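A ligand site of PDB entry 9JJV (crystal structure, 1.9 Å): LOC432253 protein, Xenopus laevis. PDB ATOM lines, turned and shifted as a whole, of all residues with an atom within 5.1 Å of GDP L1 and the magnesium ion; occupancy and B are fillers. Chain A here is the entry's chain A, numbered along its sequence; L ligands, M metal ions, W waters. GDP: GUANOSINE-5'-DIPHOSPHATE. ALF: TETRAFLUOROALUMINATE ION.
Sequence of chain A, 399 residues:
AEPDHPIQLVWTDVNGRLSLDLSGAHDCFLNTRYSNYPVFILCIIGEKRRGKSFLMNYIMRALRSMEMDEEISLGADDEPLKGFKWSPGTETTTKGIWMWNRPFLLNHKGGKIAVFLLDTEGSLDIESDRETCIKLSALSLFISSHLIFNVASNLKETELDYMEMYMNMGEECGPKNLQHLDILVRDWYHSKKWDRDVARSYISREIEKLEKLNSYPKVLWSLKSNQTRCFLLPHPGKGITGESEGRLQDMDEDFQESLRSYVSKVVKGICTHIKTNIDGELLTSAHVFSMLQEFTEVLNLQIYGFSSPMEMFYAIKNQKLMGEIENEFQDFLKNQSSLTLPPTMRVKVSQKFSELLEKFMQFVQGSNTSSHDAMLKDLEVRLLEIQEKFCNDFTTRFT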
ATOM      1  N   GLU A  47     -14.095  12.859 -16.227  1.00  0.00           N
ATOM      2  CA  GLU A  47     -13.404  12.633 -14.973  1.00  0.00           C
ATOM      3  C   GLU A  47     -11.894  12.541 -15.171  1.00  0.00           C
ATOM      4  O   GLU A  47     -11.393  12.094 -16.213  1.00  0.00           O
ATOM      5  CB  GLU A  47     -13.992  11.371 -14.304  1.00  0.00           C
ATOM      6  CG  GLU A  47     -13.063  10.521 -13.450  1.00  0.00           C
ATOM      7  CD  GLU A  47     -13.743   9.252 -12.869  1.00  0.00           C
ATOM      8  OE1 GLU A  47     -14.957   9.019 -13.092  1.00  0.00           O
ATOM      9  OE2 GLU A  47     -13.044   8.443 -12.228  1.00  0.00           O
ATOM     10  N   LYS A  48     -11.165  13.016 -14.155  1.00  0.00           N
ATOM     11  CA  LYS A  48      -9.706  13.030 -14.143  1.00  0.00           C
ATOM     12  C   LYS A  48      -9.123  11.623 -14.284  1.00  0.00           C
ATOM     13  O   LYS A  48      -9.760  10.618 -13.954  1.00  0.00           O
ATOM     14  CB  LYS A  48      -9.181  13.658 -12.862  1.00  0.00           C
ATOM     15  CG  LYS A  48      -9.471  12.777 -11.640  1.00  0.00           C
ATOM     16  CD  LYS A  48      -8.908  13.344 -10.343  1.00  0.00           C
ATOM     17  CE  LYS A  48      -9.400  12.493  -9.176  1.00  0.00           C
ATOM     18  NZ  LYS A  48      -8.337  12.054  -8.297  1.00  0.00           N
ATOM     19  N   ARG A  49      -7.863  11.570 -14.743  1.00  0.00           N
ATOM     20  CA  ARG A  49      -7.039  10.359 -14.717  1.00  0.00           C
ATOM     21  C   ARG A  49      -7.700   9.197 -15.451  1.00  0.00           C
ATOM     22  O   ARG A  49      -7.801   8.078 -14.932  1.00  0.00           O
ATOM     23  CB  ARG A  49      -6.671   9.955 -13.275  1.00  0.00           C
ATOM     24  CG  ARG A  49      -6.235  11.109 -12.358  1.00  0.00           C
ATOM     25  CD  ARG A  49      -4.740  11.391 -12.491  1.00  0.00           C
ATOM     26  NE  ARG A  49      -4.396  11.972 -13.787  1.00  0.00           N
ATOM     27  CZ  ARG A  49      -3.436  11.514 -14.583  1.00  0.00           C
ATOM     28  NH1 ARG A  49      -2.711  10.469 -14.249  1.00  0.00           N
ATOM     29  NH2 ARG A  49      -3.190  12.148 -15.737  1.00  0.00           N
ATOM     30  N   ARG A  50      -8.164   9.447 -16.665  1.00  0.00           N
ATOM     31  CA  ARG A  50      -8.786   8.339 -17.396  1.00  0.00           C
ATOM     32  C   ARG A  50      -8.420   8.371 -18.879  1.00  0.00           C
ATOM     33  O   ARG A  50      -9.233   8.024 -19.743  1.00  0.00           O
ATOM     34  CB  ARG A  50     -10.311   8.342 -17.180  1.00  0.00           C
ATOM     35  CG  ARG A  50     -10.979   6.969 -17.438  1.00  0.00           C
ATOM     36  CD  ARG A  50     -10.248   5.767 -16.780  1.00  0.00           C
ATOM     37  NE  ARG A  50     -10.161   5.962 -15.326  1.00  0.00           N
ATOM     38  CZ  ARG A  50     -10.697   5.166 -14.419  1.00  0.00           C
ATOM     39  NH1 ARG A  50     -11.234   3.984 -14.747  1.00  0.00           N
ATOM     40  NH2 ARG A  50     -10.740   5.568 -13.146  1.00  0.00           N
ATOM     41  N   GLY A  51      -7.194   8.770 -19.191  1.00  0.00           N
ATOM     42  CA  GLY A  51      -6.680   8.687 -20.559  1.00  0.00           C
ATOM     43  C   GLY A  51      -7.313   9.637 -21.567  1.00  0.00           C
ATOM     44  O   GLY A  51      -7.413   9.301 -22.756  1.00  0.00           O
ATOM     45  N   LYS A  52      -7.746  10.814 -21.125  1.00  0.00           N
ATOM     46  CA  LYS A  52      -8.268  11.808 -22.062  1.00  0.00           C
ATOM     47  C   LYS A  52      -7.136  12.353 -22.946  1.00  0.00           C
ATOM     48  O   LYS A  52      -7.259  12.385 -24.169  1.00  0.00           O
ATOM     49  CB  LYS A  52      -8.927  12.959 -21.307  1.00  0.00           C
ATOM     50  CG  LYS A  52     -10.213  12.552 -20.561  1.00  0.00           C
ATOM     51  CD  LYS A  52     -10.943  13.775 -20.034  1.00  0.00           C
ATOM     52  CE  LYS A  52     -10.087  14.554 -19.054  1.00  0.00           C
ATOM     53  NZ  LYS A  52      -9.575  13.754 -17.888  1.00  0.00           N
ATOM     54  N   SER A  53      -6.061  12.836 -22.323  1.00  0.00           N
ATOM     55  CA  SER A  53      -4.949  13.347 -23.096  1.00  0.00           C
ATOM     56  C   SER A  53      -4.353  12.254 -23.945  1.00  0.00           C
ATOM     57  O   SER A  53      -3.945  12.486 -25.086  1.00  0.00           O
ATOM     58  CB  SER A  53      -3.889  13.915 -22.148  1.00  0.00           C
ATOM     59  OG  SER A  53      -4.437  15.005 -21.431  1.00  0.00           O
ATOM     60  N   PHE A  54      -4.267  11.056 -23.374  1.00  0.00           N
ATOM     61  CA  PHE A  54      -3.752   9.889 -24.071  1.00  0.00           C
ATOM     62  C   PHE A  54      -4.546   9.638 -25.339  1.00  0.00           C
ATOM     63  O   PHE A  54      -3.976   9.432 -26.405  1.00  0.00           O
ATOM     64  CB  PHE A  54      -3.830   8.693 -23.106  1.00  0.00           C
ATOM     65  CG  PHE A  54      -3.420   7.356 -23.708  1.00  0.00           C
ATOM     66  CD1 PHE A  54      -4.291   6.645 -24.510  1.00  0.00           C
ATOM     67  CD2 PHE A  54      -2.208   6.800 -23.384  1.00  0.00           C
ATOM     68  CE1 PHE A  54      -3.941   5.421 -25.029  1.00  0.00           C
ATOM     69  CE2 PHE A  54      -1.836   5.551 -23.902  1.00  0.00           C
ATOM     70  CZ  PHE A  54      -2.707   4.860 -24.715  1.00  0.00           C
ATOM     71  N   LEU A  55      -5.880   9.678 -25.229  1.00  0.00           N
ATOM     72  CA  LEU A  55      -6.737   9.443 -26.388  1.00  0.00           C
ATOM     73  C   LEU A  55      -6.561  10.553 -27.414  1.00  0.00           C
ATOM     74  O   LEU A  55      -6.472  10.270 -28.618  1.00  0.00           O
ATOM     75  CB  LEU A  55      -8.204   9.350 -25.966  1.00  0.00           C
ATOM     76  CG  LEU A  55      -9.171   9.352 -27.158  1.00  0.00           C
ATOM     77  CD1 LEU A  55      -8.991   8.135 -28.121  1.00  0.00           C
ATOM     78  CD2 LEU A  55     -10.595   9.463 -26.654  1.00  0.00           C
ATOM     79  N   LYS A  85       0.418  16.445 -22.936  1.00  0.00           N
ATOM     80  CA  LYS A  85       1.087  15.802 -21.819  1.00  0.00           C
ATOM     81  C   LYS A  85       0.141  14.829 -21.119  1.00  0.00           C
ATOM     82  O   LYS A  85      -0.986  15.194 -20.752  1.00  0.00           O
ATOM     83  CB  LYS A  85       1.611  16.866 -20.866  1.00  0.00           C
ATOM     84  CG  LYS A  85       2.260  16.314 -19.619  1.00  0.00           C
ATOM     85  CD  LYS A  85       3.210  17.394 -19.014  1.00  0.00           C
ATOM     86  CE  LYS A  85       2.792  17.819 -17.595  1.00  0.00           C
ATOM     87  NZ  LYS A  85       1.772  18.954 -17.599  1.00  0.00           N
ATOM     88  N   TRP A  86       0.603  13.589 -20.958  1.00  0.00           N
ATOM     89  CA  TRP A  86      -0.183  12.505 -20.385  1.00  0.00           C
ATOM     90  C   TRP A  86       0.717  11.732 -19.414  1.00  0.00           C
ATOM     91  O   TRP A  86       1.928  11.635 -19.609  1.00  0.00           O
ATOM     92  CB  TRP A  86      -0.751  11.591 -21.497  1.00  0.00           C
ATOM     93  CG  TRP A  86       0.337  10.816 -22.238  1.00  0.00           C
ATOM     94  CD1 TRP A  86       1.116  11.269 -23.256  1.00  0.00           C
ATOM     95  CD2 TRP A  86       0.748   9.462 -21.986  1.00  0.00           C
ATOM     96  NE1 TRP A  86       2.006  10.282 -23.651  1.00  0.00           N
ATOM     97  CE2 TRP A  86       1.790   9.165 -22.892  1.00  0.00           C
ATOM     98  CE3 TRP A  86       0.347   8.480 -21.077  1.00  0.00           C
ATOM     99  CZ2 TRP A  86       2.424   7.926 -22.924  1.00  0.00           C
ATOM    100  CZ3 TRP A  86       0.975   7.249 -21.105  1.00  0.00           C
ATOM    101  CH2 TRP A  86       2.005   6.985 -22.014  1.00  0.00           C
ATOM    102  N   SER A  87       0.140  11.182 -18.340  1.00  0.00           N
ATOM    103  CA  SER A  87       1.017  10.664 -17.294  1.00  0.00           C
ATOM    104  C   SER A  87       0.249   9.659 -16.443  1.00  0.00           C
ATOM    105  O   SER A  87      -0.939   9.838 -16.216  1.00  0.00           O
ATOM    106  CB  SER A  87       1.528  11.811 -16.412  1.00  0.00           C
ATOM    107  OG  SER A  87       2.585  11.370 -15.562  1.00  0.00           O
ATOM    108  N   PRO A  88       0.922   8.638 -15.924  1.00  0.00           N
ATOM    109  CA  PRO A  88       0.226   7.615 -15.116  1.00  0.00           C
ATOM    110  C   PRO A  88       0.064   8.038 -13.669  1.00  0.00           C
ATOM    111  O   PRO A  88       0.717   8.950 -13.160  1.00  0.00           O
ATOM    112  CB  PRO A  88       1.147   6.398 -15.221  1.00  0.00           C
ATOM    113  CG  PRO A  88       2.519   7.011 -15.305  1.00  0.00           C
ATOM    114  CD  PRO A  88       2.325   8.262 -16.170  1.00  0.00           C
ATOM    115  N   GLY A  89      -0.821   7.331 -12.976  1.00  0.00           N
ATOM    116  CA  GLY A  89      -0.921   7.470 -11.547  1.00  0.00           C
ATOM    117  C   GLY A  89      -2.034   8.415 -11.128  1.00  0.00           C
ATOM    118  O   GLY A  89      -2.908   8.818 -11.909  1.00  0.00           O
ATOM    119  N   THR A  93      -2.641  15.941 -14.299  1.00  0.00           N
ATOM    120  CA  THR A  93      -1.662  16.483 -15.235  1.00  0.00           C
ATOM    121  C   THR A  93      -2.228  17.659 -16.018  1.00  0.00           C
ATOM    122  O   THR A  93      -1.717  18.781 -15.889  1.00  0.00           O
ATOM    123  CB  THR A  93      -1.179  15.360 -16.183  1.00  0.00           C
ATOM    124  OG1 THR A  93      -0.502  14.370 -15.415  1.00  0.00           O
ATOM    125  CG2 THR A  93      -0.263  15.899 -17.274  1.00  0.00           C
ATOM    126  N   THR A  94      -3.272  17.466 -16.810  1.00  0.00           N
ATOM    127  CA  THR A  94      -3.890  18.595 -17.503  1.00  0.00           C
ATOM    128  C   THR A  94      -4.588  19.533 -16.533  1.00  0.00           C
ATOM    129  O   THR A  94      -5.443  19.112 -15.751  1.00  0.00           O
ATOM    130  CB  THR A  94      -4.872  18.085 -18.550  1.00  0.00           C
ATOM    131  OG1 THR A  94      -4.244  17.047 -19.306  1.00  0.00           O
ATOM    132  CG2 THR A  94      -5.348  19.199 -19.496  1.00  0.00           C
ATOM    133  N   ASP A 119      -8.086  19.937 -25.121  1.00  0.00           N
ATOM    134  CA  ASP A 119      -7.852  18.926 -24.094  1.00  0.00           C
ATOM    135  C   ASP A 119      -8.127  19.581 -22.750  1.00  0.00           C
ATOM    136  O   ASP A 119      -7.477  20.577 -22.426  1.00  0.00           O
ATOM    137  CB  ASP A 119      -6.400  18.451 -24.139  1.00  0.00           C
ATOM    138  CG  ASP A 119      -6.124  17.290 -23.203  1.00  0.00           C
ATOM    139  OD1 ASP A 119      -7.065  16.566 -22.804  1.00  0.00           O
ATOM    140  OD2 ASP A 119      -4.916  17.037 -22.943  1.00  0.00           O
ATOM    141  N   THR A 120      -9.065  19.034 -21.975  1.00  0.00           N
ATOM    142  CA  THR A 120      -9.547  19.723 -20.777  1.00  0.00           C
ATOM    143  C   THR A 120      -9.115  18.976 -19.518  1.00  0.00           C
ATOM    144  O   THR A 120      -9.107  17.752 -19.479  1.00  0.00           O
ATOM    145  CB  THR A 120     -11.084  19.861 -20.801  1.00  0.00           C
ATOM    146  OG1 THR A 120     -11.507  20.399 -22.064  1.00  0.00           O
ATOM    147  CG2 THR A 120     -11.602  20.797 -19.683  1.00  0.00           C
ATOM    148  N   ARG A 186     -14.818   4.368 -21.121  1.00  0.00           N
ATOM    149  CA  ARG A 186     -13.534   3.714 -20.968  1.00  0.00           C
ATOM    150  C   ARG A 186     -13.626   2.580 -19.960  1.00  0.00           C
ATOM    151  O   ARG A 186     -14.529   2.569 -19.120  1.00  0.00           O
ATOM    152  CB  ARG A 186     -12.480   4.728 -20.525  1.00  0.00           C
ATOM    153  CG  ARG A 186     -12.503   5.982 -21.386  1.00  0.00           C
ATOM    154  CD  ARG A 186     -11.926   5.673 -22.753  1.00  0.00           C
ATOM    155  NE  ARG A 186     -10.471   5.531 -22.733  1.00  0.00           N
ATOM    156  CZ  ARG A 186      -9.627   6.539 -22.940  1.00  0.00           C
ATOM    157  NH1 ARG A 186     -10.065   7.770 -23.152  1.00  0.00           N
ATOM    158  NH2 ARG A 186      -8.324   6.303 -22.978  1.00  0.00           N
ATOM    159  N   ASP A 187     -12.710   1.608 -20.071  1.00  0.00           N
ATOM    160  CA  ASP A 187     -12.651   0.465 -19.139  1.00  0.00           C
ATOM    161  C   ASP A 187     -13.975  -0.283 -19.066  1.00  0.00           C
ATOM    162  O   ASP A 187     -14.374  -0.765 -18.000  1.00  0.00           O
ATOM    163  CB  ASP A 187     -12.212   0.916 -17.750  1.00  0.00           C
ATOM    164  CG  ASP A 187     -10.904   1.670 -17.782  1.00  0.00           C
ATOM    165  OD1 ASP A 187     -10.229   1.589 -18.834  1.00  0.00           O
ATOM    166  OD2 ASP A 187     -10.567   2.339 -16.781  1.00  0.00           O
ATOM    167  N   PRO A 234     -12.951  -1.347 -24.149  1.00  0.00           N
ATOM    168  CA  PRO A 234     -12.524  -2.190 -23.019  1.00  0.00           C
ATOM    169  C   PRO A 234     -11.291  -1.610 -22.333  1.00  0.00           C
ATOM    170  O   PRO A 234     -10.692  -0.638 -22.780  1.00  0.00           O
ATOM    171  CB  PRO A 234     -12.247  -3.562 -23.665  1.00  0.00           C
ATOM    172  CG  PRO A 234     -12.299  -3.361 -25.125  1.00  0.00           C
ATOM    173  CD  PRO A 234     -13.099  -2.112 -25.388  1.00  0.00           C
ATOM    174  N   HIS A 235     -10.944  -2.210 -21.209  1.00  0.00           N
ATOM    175  CA  HIS A 235      -9.783  -1.792 -20.425  1.00  0.00           C
ATOM    176  C   HIS A 235      -8.480  -2.024 -21.194  1.00  0.00           C
ATOM    177  O   HIS A 235      -8.294  -3.086 -21.810  1.00  0.00           O
ATOM    178  CB  HIS A 235      -9.765  -2.582 -19.098  1.00  0.00           C
ATOM    179  CG  HIS A 235      -8.832  -2.025 -18.081  1.00  0.00           C
ATOM    180  ND1 HIS A 235      -7.480  -2.271 -18.111  1.00  0.00           N
ATOM    181  CD2 HIS A 235      -9.053  -1.223 -17.012  1.00  0.00           C
ATOM    182  CE1 HIS A 235      -6.904  -1.641 -17.089  1.00  0.00           C
ATOM    183  NE2 HIS A 235      -7.837  -1.005 -16.407  1.00  0.00           N
ATOM    184  N   PRO A 236      -7.541  -1.078 -21.157  1.00  0.00           N
ATOM    185  CA  PRO A 236      -6.314  -1.210 -21.965  1.00  0.00           C
ATOM    186  C   PRO A 236      -5.279  -2.147 -21.381  1.00  0.00           C
ATOM    187  O   PRO A 236      -4.325  -2.508 -22.089  1.00  0.00           O
ATOM    188  CB  PRO A 236      -5.779   0.230 -22.012  1.00  0.00           C
ATOM    189  CG  PRO A 236      -6.233   0.787 -20.659  1.00  0.00           C
ATOM    190  CD  PRO A 236      -7.591   0.206 -20.441  1.00  0.00           C
ATOM    191  N   ILE A 240      -0.599  -0.392 -20.188  1.00  0.00           N
ATOM    192  CA  ILE A 240      -0.926   0.992 -20.455  1.00  0.00           C
ATOM    193  C   ILE A 240      -1.142   1.791 -19.175  1.00  0.00           C
ATOM    194  O   ILE A 240      -0.837   2.992 -19.144  1.00  0.00           O
ATOM    195  CB  ILE A 240      -2.156   1.074 -21.380  1.00  0.00           C
ATOM    196  CG1 ILE A 240      -1.790   0.603 -22.786  1.00  0.00           C
ATOM    197  CG2 ILE A 240      -2.757   2.496 -21.416  1.00  0.00           C
ATOM    198  CD1 ILE A 240      -0.904   1.597 -23.581  1.00  0.00           C
ATOM    199  N   THR A 241      -1.637   1.173 -18.089  1.00  0.00           N
ATOM    200  CA  THR A 241      -1.956   1.976 -16.906  1.00  0.00           C
ATOM    201  C   THR A 241      -0.769   2.186 -15.976  1.00  0.00           C
ATOM    202  O   THR A 241      -0.800   3.123 -15.171  1.00  0.00           O
ATOM    203  CB  THR A 241      -3.112   1.384 -16.093  1.00  0.00           C
ATOM    204  OG1 THR A 241      -2.721   0.146 -15.507  1.00  0.00           O
ATOM    205  CG2 THR A 241      -4.334   1.199 -16.964  1.00  0.00           C
ATOM    206  N   GLY A 242       0.251   1.361 -16.068  1.00  0.00           N
ATOM    207  CA  GLY A 242       1.451   1.530 -15.270  1.00  0.00           C
ATOM    208  C   GLY A 242       2.467   2.387 -15.987  1.00  0.00           C
ATOM    209  O   GLY A 242       2.140   3.183 -16.872  1.00  0.00           O
ATOM    210  N   PHE A 255      -8.721  -3.677 -26.416  1.00  0.00           N
ATOM    211  CA  PHE A 255      -8.650  -2.220 -26.351  1.00  0.00           C
ATOM    212  C   PHE A 255      -8.151  -1.649 -27.670  1.00  0.00           C
ATOM    213  O   PHE A 255      -8.750  -0.708 -28.215  1.00  0.00           O
ATOM    214  CB  PHE A 255      -7.732  -1.796 -25.209  1.00  0.00           C
ATOM    215  CG  PHE A 255      -7.483  -0.315 -25.146  1.00  0.00           C
ATOM    216  CD1 PHE A 255      -8.484   0.548 -24.675  1.00  0.00           C
ATOM    217  CD2 PHE A 255      -6.276   0.228 -25.574  1.00  0.00           C
ATOM    218  CE1 PHE A 255      -8.267   1.924 -24.613  1.00  0.00           C
ATOM    219  CE2 PHE A 255      -6.057   1.586 -25.526  1.00  0.00           C
ATOM    220  CZ  PHE A 255      -7.045   2.445 -25.054  1.00  0.00           C
HETATM  221  PB  GDP L   1      -6.198  12.357 -18.190  1.00  0.00           P
HETATM  222  O1B GDP L   1      -7.594  11.832 -18.399  1.00  0.00           O
HETATM  223  O2B GDP L   1      -6.061  13.136 -16.865  1.00  0.00           O
HETATM  224  O3B GDP L   1      -5.867  13.244 -19.342  1.00  0.00           O
HETATM  225  O3A GDP L   1      -5.245  11.051 -18.211  1.00  0.00           O
HETATM  226  PA  GDP L   1      -3.980  10.772 -19.147  1.00  0.00           P
HETATM  227  O1A GDP L   1      -2.860  11.642 -18.599  1.00  0.00           O
HETATM  228  O2A GDP L   1      -4.184  10.882 -20.623  1.00  0.00           O
HETATM  229  O5' GDP L   1      -3.721   9.239 -18.797  1.00  0.00           O
HETATM  230  C5' GDP L   1      -3.675   8.859 -17.414  1.00  0.00           C
HETATM  231  C4' GDP L   1      -3.197   7.406 -17.363  1.00  0.00           C
HETATM  232  O4' GDP L   1      -4.254   6.639 -17.915  1.00  0.00           O
HETATM  233  C3' GDP L   1      -1.980   7.087 -18.216  1.00  0.00           C
HETATM  234  O3' GDP L   1      -1.157   6.147 -17.492  1.00  0.00           O
HETATM  235  C2' GDP L   1      -2.584   6.411 -19.441  1.00  0.00           C
HETATM  236  O2' GDP L   1      -1.676   5.572 -20.133  1.00  0.00           O
HETATM  237  C1' GDP L   1      -3.739   5.658 -18.806  1.00  0.00           C
HETATM  238  N9  GDP L   1      -4.816   5.320 -19.750  1.00  0.00           N
HETATM  239  C8  GDP L   1      -4.938   5.620 -21.063  1.00  0.00           C
HETATM  240  N7  GDP L   1      -6.093   5.102 -21.556  1.00  0.00           N
HETATM  241  C5  GDP L   1      -6.741   4.499 -20.534  1.00  0.00           C
HETATM  242  C6  GDP L   1      -7.997   3.762 -20.339  1.00  0.00           C
HETATM  243  O6  GDP L   1      -8.773   3.576 -21.302  1.00  0.00           O
HETATM  244  N1  GDP L   1      -8.277   3.272 -19.122  1.00  0.00           N
HETATM  245  C2  GDP L   1      -7.446   3.441 -18.077  1.00  0.00           C
HETATM  246  N2  GDP L   1      -7.770   2.923 -16.870  1.00  0.00           N
HETATM  247  N3  GDP L   1      -6.273   4.099 -18.190  1.00  0.00           N
HETATM  248  C4  GDP L   1      -5.892   4.638 -19.362  1.00  0.00           C
HETATM  249 AL   ALF L   2      -6.159  14.690 -16.161  1.00  0.00          AL
HETATM  250  F1  ALF L   2      -7.902  14.686 -16.403  1.00  0.00           F
HETATM  251  F2  ALF L   2      -4.395  14.740 -15.825  1.00  0.00           F
HETATM  252  F3  ALF L   2      -6.304  13.915 -14.586  1.00  0.00           F
HETATM  253  F4  ALF L   2      -5.927  15.506 -17.742  1.00  0.00           F
HETATM  254 MG    MG M   1      -5.119  15.081 -19.480  1.00  0.00          MG
HETATM  255  O   HOH W   1      -6.838  15.954 -20.127  1.00  0.00           O
HETATM  256  O   HOH W   2     -10.791   2.069 -22.025  1.00  0.00           O
HETATM  257  O   HOH W   3       1.135   5.172 -18.472  1.00  0.00           O
HETATM  258  O   HOH W   4      -3.319  14.281 -18.907  1.00  0.00           O
HETATM  259  O   HOH W   5      -4.827   4.825 -15.589  1.00  0.00           O
HETATM  260  O   HOH W   6      -6.021   2.735 -14.297  1.00  0.00           O
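O1B of GDP L1 sits at hydrogen-bond distance from N of Arg 50 (3.0 Å).
N of Arg 49 sits close to O2B of GDP L1 (3.2 Å).
A fluorine (F3) of ALF L2 sits at hydrogen-bond distance from the guanidinium group (NE) of Arg 49 (2.8 Å).
The side-chain amino group of Lys 52 lies within hydrogen-bond range of a fluorine (F1) of ALF L2 (2.4 Å).
The side-chain carboxylate (OD1) of Asp 187 sits at hydrogen-bond distance from a nitrogen (N1) of GDP L1 (2.6 Å).
An oxygen (O3A) of GDP L1 is in hydrogen-bond range of the backbone NH (N) of Gly 51 (3.2 Å).
An oxygen (O1A) of GDP L1 is in salt-bridge range of the guanidinium group (NH2) of Arg 49 (2.9 Å).
N of Thr 93 is in hydrogen-bond range of F2 of ALF L2 (2.6 Å).
An oxygen (O2A) of GDP L1 lies within hydrogen-bond range of the backbone NH of Ser 53 (3.2 Å).
The backbone NH of Phe 54 sits at hydrogen-bond distance from an oxygen (O2A) of GDP L1 (2.8 Å).
The backbone NH (N) of Lys 52 sits at hydrogen-bond distance from an oxygen (O1B) of GDP L1 (2.9 Å).
O1B of GDP L1 lies within salt-bridge range of NZ of Lys 52.
The backbone NH (N) of Ser 87 lies within hydrogen-bond range of an oxygen (O1A) of GDP L1 (3.0 Å).
A fluorine (F2) of ALF L2 sits at hydrogen-bond distance from the backbone NH (N) of Thr 94.
N of Arg 49 is in hydrogen-bond range of F3 of ALF L2 (2.8 Å).
The backbone carbonyl oxygen (O) of Ile 240 sits at hydrogen-bond distance from an oxygen (O2') of GDP L1 (2.9 Å).
The guanidinium group (NH2) of Arg 186 is in hydrogen-bond range of a nitrogen (N7) of GDP L1.
An oxygen (O2B) of GDP L1 is bound to an aluminium atom (AL) of ALF L2.
O of Ser 87 sits at hydrogen-bond distance from NH1 of Arg 49, at 2.7 Å.
The guanidinium group (NH1) of Arg 50 is in salt-bridge range of the side-chain carboxylate (OD2) of Asp 187 (2.7 Å).
The backbone carbonyl oxygen of Glu 47 lies within hydrogen-bond range of the side-chain amino group of Lys 52 (3.0 Å).
The guanidinium group (NH1) of Arg 49 sits at hydrogen-bond distance from the backbone carbonyl oxygen (O) of Gly 89 (2.9 Å).
The side-chain hydroxyl of Ser 53 lies close to the side-chain carboxylate of Asp 119 (2.6 Å).
The backbone carbonyl oxygen (O) of Gly 51 lies within hydrogen-bond range of the guanidinium group (NH1) of Arg 186 (3.1 Å).
The side-chain carboxylate (OE2) of Glu 47 lies within salt-bridge range of the guanidinium group (NH2) of Arg 50 (3.8 Å).
CZ3 of Trp 86 touches O2' of GDP L1 (3.3 Å).
Pro 88 touches GDP L1.
His 235 touches GDP L1 (NE2 to N2, 3.96 Å).
CD of Pro 236 touches N1 of GDP L1 (3.4 Å).
Thr 241 touches GDP L1 (CG2 to N3, 3.7 Å).
Phe 255 touches GDP L1.
Hydrophobic or aromatic side chains that line GDP L1: Phe 54, Trp 86, Pro 88, Pro 236, Ile 240 and Phe 255.
Within 4 Å of GDP L1: Arg 49, Arg 50, Gly 51, Lys 52, Ser 53, Phe 54, Trp 86, Ser 87, Pro 88, Arg 186, Asp 187, His 235, Pro 236, Ile 240, Thr 241 and Phe 255.
Along chain A the residues within 4 Å of GDP L1 span positions 49 to 255.
The nearest printed residue that does not touch GDP L1 is Thr 94 (4.1 Å).
Asp 119 touches the magnesium ion (OD2 to MG, 3.98 Å).
Within 4 Å of the magnesium ion: Ser 53, Thr 94 and Asp 119.
The nearest printed residue that does not touch the magnesium ion is Lys 85 (4.3 Å).
The magnesium ion is bound by F4 of ALF L2 (2.0 Å).
The magnesium ion is bound by an oxygen (O3B) of GDP L1 (2.0 Å).
The magnesium ion is bound by water W1 (2.0 Å).
Water W4 binds the magnesium ion (2.1 Å).
OG of Ser 53 binds the magnesium ion (2.1 Å).
OG1 of Thr 94 binds the magnesium ion, at 2.2 Å.
Water W4 bridges an oxygen (O1A) of GDP L1 (2.7 Å) and the backbone carbonyl oxygen (O) of Lys 85 (3.1 Å).
Water W1 lies within hydrogen-bond range of OD1 of Asp 119 and O of Thr 120.
Water W2 lies within hydrogen-bond range of an oxygen (O6) of GDP L1 (2.6 Å), the backbone NH (N) of Asp 187 (2.8 Å) and the backbone carbonyl oxygen (O) of Pro 234 (2.8 Å).
Water W3 lies within hydrogen-bond range of an oxygen (O3') of GDP L1 (2.7 Å), the backbone carbonyl oxygen of Gly 242 (2.7 Å) and the backbone carbonyl oxygen of Ile 240 (3.0 Å).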
